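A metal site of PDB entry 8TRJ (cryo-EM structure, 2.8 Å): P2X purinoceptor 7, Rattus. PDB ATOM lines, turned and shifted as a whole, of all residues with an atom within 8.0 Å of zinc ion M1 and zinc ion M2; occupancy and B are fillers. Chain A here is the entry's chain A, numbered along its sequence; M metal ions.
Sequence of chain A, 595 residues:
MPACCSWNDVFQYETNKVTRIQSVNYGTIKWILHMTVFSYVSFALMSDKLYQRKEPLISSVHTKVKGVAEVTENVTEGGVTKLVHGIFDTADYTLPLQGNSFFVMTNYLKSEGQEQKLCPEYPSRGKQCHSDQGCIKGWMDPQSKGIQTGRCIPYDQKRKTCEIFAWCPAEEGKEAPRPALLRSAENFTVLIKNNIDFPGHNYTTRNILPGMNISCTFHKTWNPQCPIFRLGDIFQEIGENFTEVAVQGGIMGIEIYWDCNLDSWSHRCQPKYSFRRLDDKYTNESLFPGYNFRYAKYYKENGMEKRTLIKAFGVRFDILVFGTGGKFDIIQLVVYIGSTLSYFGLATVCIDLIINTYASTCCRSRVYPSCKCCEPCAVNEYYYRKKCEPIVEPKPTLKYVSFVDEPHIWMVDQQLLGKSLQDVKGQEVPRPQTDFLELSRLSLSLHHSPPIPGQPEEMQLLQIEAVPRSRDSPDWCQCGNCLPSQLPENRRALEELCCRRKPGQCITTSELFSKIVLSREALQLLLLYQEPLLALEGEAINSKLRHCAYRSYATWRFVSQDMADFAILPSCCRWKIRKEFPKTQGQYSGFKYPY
SG of Cys 498 lies close to O of Arg 500, 3.7 Å away.
SG of Cys 498 lies close to N of Gln 478 (3.0 Å).
The backbone carbonyl oxygen (O) of Cys 499 is in hydrogen-bond range of the backbone NH (N) of Val 404 (3.1 Å).
The side-chain amide oxygen (OE1) of Gln 422 sits at hydrogen-bond distance from the backbone NH (N) of Cys 498, at 2.9 Å.
The side-chain sulfur (SG) of Cys 482 lies close to the backbone NH (N) of Cys 572 (3.5 Å).
SG of Cys 506 lies close to OG1 of Thr 508 (3.1 Å).
The side-chain sulfur of Cys 477 lies close to the backbone NH of Gly 480.
SG of Cys 572 lies close to SG of Cys 573, at 3.7 Å.
Four residues have an atom within 4 Å of zinc ion M1: Cys 479, Cys 499, Cys 506 and Cys 572.
Merely in contact with zinc ion M2: Gly 480 (3.7 Å) and Gln 478 (3.9 Å).
Six residues have an atom within 4 Å of zinc ion M2: Cys 477, Gln 478, Cys 479, Gly 480, Cys 482 and Cys 498.
The nearest printed residue that does not touch zinc ion M2 is Asn 481 (4.4 Å).
Zinc ion M1 is bound by the side-chain sulfur (SG) of Cys 506 (2.3 Å), the side-chain sulfur (SG) of Cys 499 (2.3 Å), the side-chain sulfur (SG) of Cys 479 (2.3 Å) and the side-chain sulfur (SG) of Cys 572 (2.3 Å).
Zinc ion M2 is bound by SG of Cys 482 (2.3 Å), SG of Cys 498 (2.3 Å), SG of Cys 477 (2.3 Å) and SG of Cys 479 (2.3 Å).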
ATOM      1  N   VAL A 404      -2.249 -26.753  -0.375  1.00  0.00           N
ATOM      2  CA  VAL A 404      -2.690 -27.737   0.603  1.00  0.00           C
ATOM      3  C   VAL A 404      -2.598 -27.131   1.986  1.00  0.00           C
ATOM      4  O   VAL A 404      -3.530 -27.237   2.787  1.00  0.00           O
ATOM      5  CB  VAL A 404      -1.842 -29.019   0.545  1.00  0.00           C
ATOM      6  CG1 VAL A 404      -2.254 -29.973   1.640  1.00  0.00           C
ATOM      7  CG2 VAL A 404      -1.958 -29.683  -0.812  1.00  0.00           C
ATOM      8  N   GLN A 422       3.084 -18.054  -7.966  1.00  0.00           N
ATOM      9  CA  GLN A 422       3.346 -18.415  -6.583  1.00  0.00           C
ATOM     10  C   GLN A 422       3.541 -17.177  -5.717  1.00  0.00           C
ATOM     11  O   GLN A 422       2.935 -17.040  -4.648  1.00  0.00           O
ATOM     12  CB  GLN A 422       4.572 -19.317  -6.506  1.00  0.00           C
ATOM     13  CG  GLN A 422       5.050 -19.674  -5.106  1.00  0.00           C
ATOM     14  CD  GLN A 422       4.136 -20.650  -4.402  1.00  0.00           C
ATOM     15  OE1 GLN A 422       3.977 -21.798  -4.834  1.00  0.00           O
ATOM     16  NE2 GLN A 422       3.540 -20.211  -3.302  1.00  0.00           N
ATOM     17  N   SER A 473      14.038 -28.377  -7.510  1.00  0.00           N
ATOM     18  CA  SER A 473      13.352 -27.480  -6.573  1.00  0.00           C
ATOM     19  C   SER A 473      13.533 -26.028  -6.984  1.00  0.00           C
ATOM     20  O   SER A 473      14.419 -25.347  -6.474  1.00  0.00           O
ATOM     21  CB  SER A 473      13.858 -27.696  -5.154  1.00  0.00           C
ATOM     22  OG  SER A 473      13.660 -29.031  -4.729  1.00  0.00           O
ATOM     23  N   PRO A 474      12.684 -25.539  -7.900  1.00  0.00           N
ATOM     24  CA  PRO A 474      12.735 -24.110  -8.252  1.00  0.00           C
ATOM     25  C   PRO A 474      12.652 -23.206  -7.029  1.00  0.00           C
ATOM     26  O   PRO A 474      12.236 -23.649  -5.945  1.00  0.00           O
ATOM     27  CB  PRO A 474      11.516 -23.948  -9.168  1.00  0.00           C
ATOM     28  CG  PRO A 474      11.293 -25.294  -9.724  1.00  0.00           C
ATOM     29  CD  PRO A 474      11.633 -26.247  -8.631  1.00  0.00           C
ATOM     30  N   TRP A 476      10.639 -21.041  -6.227  1.00  0.00           N
ATOM     31  CA  TRP A 476       9.266 -20.930  -5.736  1.00  0.00           C
ATOM     32  C   TRP A 476       8.689 -22.255  -5.280  1.00  0.00           C
ATOM     33  O   TRP A 476       7.522 -22.307  -4.871  1.00  0.00           O
ATOM     34  CB  TRP A 476       8.364 -20.327  -6.816  1.00  0.00           C
ATOM     35  CG  TRP A 476       8.587 -20.842  -8.202  1.00  0.00           C
ATOM     36  CD1 TRP A 476       9.206 -20.195  -9.220  1.00  0.00           C
ATOM     37  CD2 TRP A 476       8.186 -22.124  -8.712  1.00  0.00           C
ATOM     38  NE1 TRP A 476       9.216 -20.988 -10.345  1.00  0.00           N
ATOM     39  CE2 TRP A 476       8.598 -22.181 -10.056  1.00  0.00           C
ATOM     40  CE3 TRP A 476       7.517 -23.222  -8.165  1.00  0.00           C
ATOM     41  CZ2 TRP A 476       8.371 -23.286 -10.868  1.00  0.00           C
ATOM     42  CZ3 TRP A 476       7.299 -24.322  -8.968  1.00  0.00           C
ATOM     43  CH2 TRP A 476       7.715 -24.343 -10.305  1.00  0.00           C
ATOM     44  N   CYS A 477       9.465 -23.337  -5.317  1.00  0.00           N
ATOM     45  CA  CYS A 477       8.971 -24.666  -4.987  1.00  0.00           C
ATOM     46  C   CYS A 477       9.263 -25.008  -3.537  1.00  0.00           C
ATOM     47  O   CYS A 477      10.397 -24.855  -3.068  1.00  0.00           O
ATOM     48  CB  CYS A 477       9.592 -25.712  -5.900  1.00  0.00           C
ATOM     49  SG  CYS A 477       9.117 -27.404  -5.508  1.00  0.00           S
ATOM     50  N   GLN A 478       8.230 -25.468  -2.828  1.00  0.00           N
ATOM     51  CA  GLN A 478       8.365 -25.956  -1.461  1.00  0.00           C
ATOM     52  C   GLN A 478       8.186 -27.462  -1.358  1.00  0.00           C
ATOM     53  O   GLN A 478       8.392 -28.022  -0.271  1.00  0.00           O
ATOM     54  CB  GLN A 478       7.342 -25.265  -0.553  1.00  0.00           C
ATOM     55  CG  GLN A 478       7.737 -23.874  -0.100  1.00  0.00           C
ATOM     56  CD  GLN A 478       7.524 -22.817  -1.177  1.00  0.00           C
ATOM     57  OE1 GLN A 478       7.822 -23.033  -2.344  1.00  0.00           O
ATOM     58  NE2 GLN A 478       7.014 -21.658  -0.768  1.00  0.00           N
ATOM     59  N   CYS A 479       7.804 -28.136  -2.439  1.00  0.00           N
ATOM     60  CA  CYS A 479       7.568 -29.574  -2.427  1.00  0.00           C
ATOM     61  C   CYS A 479       8.709 -30.373  -3.044  1.00  0.00           C
ATOM     62  O   CYS A 479       8.917 -31.535  -2.652  1.00  0.00           O
ATOM     63  CB  CYS A 479       6.276 -29.901  -3.167  1.00  0.00           C
ATOM     64  SG  CYS A 479       6.428 -29.955  -4.969  1.00  0.00           S
ATOM     65  N   GLY A 480       9.443 -29.798  -3.983  1.00  0.00           N
ATOM     66  CA  GLY A 480      10.589 -30.435  -4.590  1.00  0.00           C
ATOM     67  C   GLY A 480      10.305 -31.177  -5.883  1.00  0.00           C
ATOM     68  O   GLY A 480      11.246 -31.441  -6.642  1.00  0.00           O
ATOM     69  N   ASN A 481       9.044 -31.507  -6.163  1.00  0.00           N
ATOM     70  CA  ASN A 481       8.700 -32.211  -7.385  1.00  0.00           C
ATOM     71  C   ASN A 481       8.339 -31.270  -8.527  1.00  0.00           C
ATOM     72  O   ASN A 481       8.110 -31.749  -9.648  1.00  0.00           O
ATOM     73  CB  ASN A 481       7.525 -33.161  -7.130  1.00  0.00           C
ATOM     74  CG  ASN A 481       7.345 -34.171  -8.251  1.00  0.00           C
ATOM     75  OD1 ASN A 481       8.178 -34.259  -9.156  1.00  0.00           O
ATOM     76  ND2 ASN A 481       6.274 -34.945  -8.194  1.00  0.00           N
ATOM     77  N   CYS A 482       8.285 -29.971  -8.283  1.00  0.00           N
ATOM     78  CA  CYS A 482       7.965 -29.028  -9.347  1.00  0.00           C
ATOM     79  C   CYS A 482       9.092 -28.959 -10.357  1.00  0.00           C
ATOM     80  O   CYS A 482      10.254 -28.771  -9.993  1.00  0.00           O
ATOM     81  CB  CYS A 482       7.690 -27.645  -8.775  1.00  0.00           C
ATOM     82  SG  CYS A 482       6.134 -27.506  -7.853  1.00  0.00           S
ATOM     83  N   LEU A 483       8.767 -29.119 -11.634  1.00  0.00           N
ATOM     84  CA  LEU A 483       9.751 -29.004 -12.690  1.00  0.00           C
ATOM     85  C   LEU A 483       9.694 -27.607 -13.285  1.00  0.00           C
ATOM     86  O   LEU A 483       8.598 -27.035 -13.409  1.00  0.00           O
ATOM     87  CB  LEU A 483       9.500 -30.029 -13.786  1.00  0.00           C
ATOM     88  CG  LEU A 483       9.233 -31.471 -13.381  1.00  0.00           C
ATOM     89  CD1 LEU A 483       9.204 -32.357 -14.609  1.00  0.00           C
ATOM     90  CD2 LEU A 483      10.271 -31.980 -12.384  1.00  0.00           C
ATOM     91  N   LEU A 497       4.263 -22.348  -9.924  1.00  0.00           N
ATOM     92  CA  LEU A 497       3.368 -22.572  -8.796  1.00  0.00           C
ATOM     93  C   LEU A 497       3.727 -23.881  -8.113  1.00  0.00           C
ATOM     94  O   LEU A 497       4.164 -24.836  -8.751  1.00  0.00           O
ATOM     95  CB  LEU A 497       1.903 -22.598  -9.264  1.00  0.00           C
ATOM     96  CG  LEU A 497       0.814 -22.747  -8.190  1.00  0.00           C
ATOM     97  CD1 LEU A 497       0.705 -21.601  -7.191  1.00  0.00           C
ATOM     98  CD2 LEU A 497      -0.537 -23.169  -8.761  1.00  0.00           C
ATOM     99  N   CYS A 498       3.522 -23.917  -6.795  1.00  0.00           N
ATOM    100  CA  CYS A 498       3.795 -25.087  -5.985  1.00  0.00           C
ATOM    101  C   CYS A 498       2.514 -25.558  -5.302  1.00  0.00           C
ATOM    102  O   CYS A 498       1.617 -24.761  -5.020  1.00  0.00           O
ATOM    103  CB  CYS A 498       4.856 -24.807  -4.918  1.00  0.00           C
ATOM    104  SG  CYS A 498       5.692 -26.269  -4.292  1.00  0.00           S
ATOM    105  N   CYS A 499       2.453 -26.858  -5.048  1.00  0.00           N
ATOM    106  CA  CYS A 499       1.271 -27.436  -4.414  1.00  0.00           C
ATOM    107  C   CYS A 499       1.019 -26.846  -3.031  1.00  0.00           C
ATOM    108  O   CYS A 499      -0.120 -26.814  -2.568  1.00  0.00           O
ATOM    109  CB  CYS A 499       1.423 -28.944  -4.319  1.00  0.00           C
ATOM    110  SG  CYS A 499       2.963 -29.473  -3.570  1.00  0.00           S
ATOM    111  N   ARG A 500       2.079 -26.397  -2.356  1.00  0.00           N
ATOM    112  CA  ARG A 500       1.955 -25.819  -1.020  1.00  0.00           C
ATOM    113  C   ARG A 500       2.817 -24.572  -0.925  1.00  0.00           C
ATOM    114  O   ARG A 500       3.810 -24.420  -1.652  1.00  0.00           O
ATOM    115  CB  ARG A 500       2.355 -26.820   0.073  1.00  0.00           C
ATOM    116  CG  ARG A 500       3.653 -27.557  -0.195  1.00  0.00           C
ATOM    117  CD  ARG A 500       3.836 -28.702   0.779  1.00  0.00           C
ATOM    118  NE  ARG A 500       3.330 -28.389   2.123  1.00  0.00           N
ATOM    119  CZ  ARG A 500       2.867 -29.286   2.987  1.00  0.00           C
ATOM    120  NH1 ARG A 500       2.835 -30.565   2.676  1.00  0.00           N
ATOM    121  NH2 ARG A 500       2.439 -28.889   4.170  1.00  0.00           N
ATOM    122  N   GLY A 504       6.966 -29.165   2.880  1.00  0.00           N
ATOM    123  CA  GLY A 504       6.232 -30.288   3.432  1.00  0.00           C
ATOM    124  C   GLY A 504       6.011 -31.341   2.376  1.00  0.00           C
ATOM    125  O   GLY A 504       6.611 -31.321   1.297  1.00  0.00           O
ATOM    126  N   GLN A 505       5.129 -32.289   2.714  1.00  0.00           N
ATOM    127  CA  GLN A 505       4.809 -33.368   1.796  1.00  0.00           C
ATOM    128  C   GLN A 505       4.076 -32.826   0.569  1.00  0.00           C
ATOM    129  O   GLN A 505       3.190 -31.972   0.686  1.00  0.00           O
ATOM    130  CB  GLN A 505       3.961 -34.423   2.500  1.00  0.00           C
ATOM    131  CG  GLN A 505       4.777 -35.530   3.145  1.00  0.00           C
ATOM    132  CD  GLN A 505       3.905 -36.624   3.733  1.00  0.00           C
ATOM    133  OE1 GLN A 505       2.676 -36.553   3.688  1.00  0.00           O
ATOM    134  NE2 GLN A 505       4.540 -37.638   4.312  1.00  0.00           N
ATOM    135  N   CYS A 506       4.450 -33.331  -0.595  1.00  0.00           N
ATOM    136  CA  CYS A 506       3.800 -32.926  -1.838  1.00  0.00           C
ATOM    137  C   CYS A 506       2.402 -33.518  -1.924  1.00  0.00           C
ATOM    138  O   CYS A 506       2.163 -34.649  -1.499  1.00  0.00           O
ATOM    139  CB  CYS A 506       4.637 -33.363  -3.032  1.00  0.00           C
ATOM    140  SG  CYS A 506       4.011 -32.808  -4.637  1.00  0.00           S
ATOM    141  N   ILE A 507       1.467 -32.746  -2.481  1.00  0.00           N
ATOM    142  CA  ILE A 507       0.145 -33.281  -2.765  1.00  0.00           C
ATOM    143  C   ILE A 507       0.240 -34.422  -3.763  1.00  0.00           C
ATOM    144  O   ILE A 507      -0.587 -35.339  -3.761  1.00  0.00           O
ATOM    145  CB  ILE A 507      -0.785 -32.175  -3.283  1.00  0.00           C
ATOM    146  CG1 ILE A 507      -2.244 -32.600  -3.165  1.00  0.00           C
ATOM    147  CG2 ILE A 507      -0.475 -31.869  -4.724  1.00  0.00           C
ATOM    148  CD1 ILE A 507      -3.220 -31.501  -3.479  1.00  0.00           C
ATOM    149  N   THR A 508       1.251 -34.389  -4.635  1.00  0.00           N
ATOM    150  CA  THR A 508       1.354 -35.369  -5.704  1.00  0.00           C
ATOM    151  C   THR A 508       1.516 -36.779  -5.164  1.00  0.00           C
ATOM    152  O   THR A 508       0.980 -37.737  -5.727  1.00  0.00           O
ATOM    153  CB  THR A 508       2.513 -35.006  -6.624  1.00  0.00           C
ATOM    154  OG1 THR A 508       2.320 -33.681  -7.137  1.00  0.00           O
ATOM    155  CG2 THR A 508       2.598 -35.964  -7.774  1.00  0.00           C
ATOM    156  N   THR A 509       2.265 -36.928  -4.063  1.00  0.00           N
ATOM    157  CA  THR A 509       2.449 -38.245  -3.470  1.00  0.00           C
ATOM    158  C   THR A 509       1.226 -38.727  -2.720  1.00  0.00           C
ATOM    159  O   THR A 509       1.194 -39.881  -2.285  1.00  0.00           O
ATOM    160  CB  THR A 509       3.664 -38.249  -2.535  1.00  0.00           C
ATOM    161  OG1 THR A 509       3.773 -39.525  -1.900  1.00  0.00           O
ATOM    162  CG2 THR A 509       3.535 -37.159  -1.471  1.00  0.00           C
ATOM    163  N   TYR A 553      -8.261 -32.578 -11.007  1.00  0.00           N
ATOM    164  CA  TYR A 553      -7.590 -31.793  -9.980  1.00  0.00           C
ATOM    165  C   TYR A 553      -8.355 -30.504  -9.705  1.00  0.00           C
ATOM    166  O   TYR A 553      -8.634 -30.175  -8.546  1.00  0.00           O
ATOM    167  CB  TYR A 553      -6.149 -31.489 -10.390  1.00  0.00           C
ATOM    168  CG  TYR A 553      -5.346 -30.813  -9.313  1.00  0.00           C
ATOM    169  CD1 TYR A 553      -5.329 -29.434  -9.189  1.00  0.00           C
ATOM    170  CD2 TYR A 553      -4.624 -31.553  -8.395  1.00  0.00           C
ATOM    171  CE1 TYR A 553      -4.606 -28.816  -8.204  1.00  0.00           C
ATOM    172  CE2 TYR A 553      -3.895 -30.944  -7.399  1.00  0.00           C
ATOM    173  CZ  TYR A 553      -3.889 -29.571  -7.314  1.00  0.00           C
ATOM    174  OH  TYR A 553      -3.165 -28.952  -6.319  1.00  0.00           O
ATOM    175  N   PRO A 570      -0.542 -26.709 -10.077  1.00  0.00           N
ATOM    176  CA  PRO A 570       0.877 -26.576  -9.733  1.00  0.00           C
ATOM    177  C   PRO A 570       1.757 -27.313 -10.730  1.00  0.00           C
ATOM    178  O   PRO A 570       1.313 -28.214 -11.453  1.00  0.00           O
ATOM    179  CB  PRO A 570       0.964 -27.202  -8.345  1.00  0.00           C
ATOM    180  CG  PRO A 570      -0.404 -27.179  -7.818  1.00  0.00           C
ATOM    181  CD  PRO A 570      -1.296 -27.348  -8.992  1.00  0.00           C
ATOM    182  N   SER A 571       3.015 -26.903 -10.766  1.00  0.00           N
ATOM    183  CA  SER A 571       3.955 -27.491 -11.716  1.00  0.00           C
ATOM    184  C   SER A 571       4.139 -28.989 -11.453  1.00  0.00           C
ATOM    185  O   SER A 571       4.186 -29.779 -12.400  1.00  0.00           O
ATOM    186  CB  SER A 571       5.290 -26.763 -11.645  1.00  0.00           C
ATOM    187  OG  SER A 571       6.141 -27.142 -12.713  1.00  0.00           O
ATOM    188  N   CYS A 572       4.238 -29.385 -10.189  1.00  0.00           N
ATOM    189  CA  CYS A 572       4.481 -30.792  -9.875  1.00  0.00           C
ATOM    190  C   CYS A 572       3.357 -31.671 -10.420  1.00  0.00           C
ATOM    191  O   CYS A 572       3.603 -32.664 -11.115  1.00  0.00           O
ATOM    192  CB  CYS A 572       4.623 -30.975  -8.367  1.00  0.00           C
ATOM    193  SG  CYS A 572       3.348 -30.179  -7.361  1.00  0.00           S
ATOM    194  N   CYS A 573       2.114 -31.324 -10.101  1.00  0.00           N
ATOM    195  CA  CYS A 573       0.974 -32.117 -10.550  1.00  0.00           C
ATOM    196  C   CYS A 573       0.850 -32.096 -12.070  1.00  0.00           C
ATOM    197  O   CYS A 573       0.613 -33.132 -12.695  1.00  0.00           O
ATOM    198  CB  CYS A 573      -0.305 -31.585  -9.899  1.00  0.00           C
ATOM    199  SG  CYS A 573      -0.079 -31.146  -8.163  1.00  0.00           S
HETATM  200 ZN    ZN M   1       4.192 -30.564  -5.217  1.00  0.00          ZN
HETATM  201 ZN    ZN M   2       6.825 -27.767  -5.658  1.00  0.00          ZN
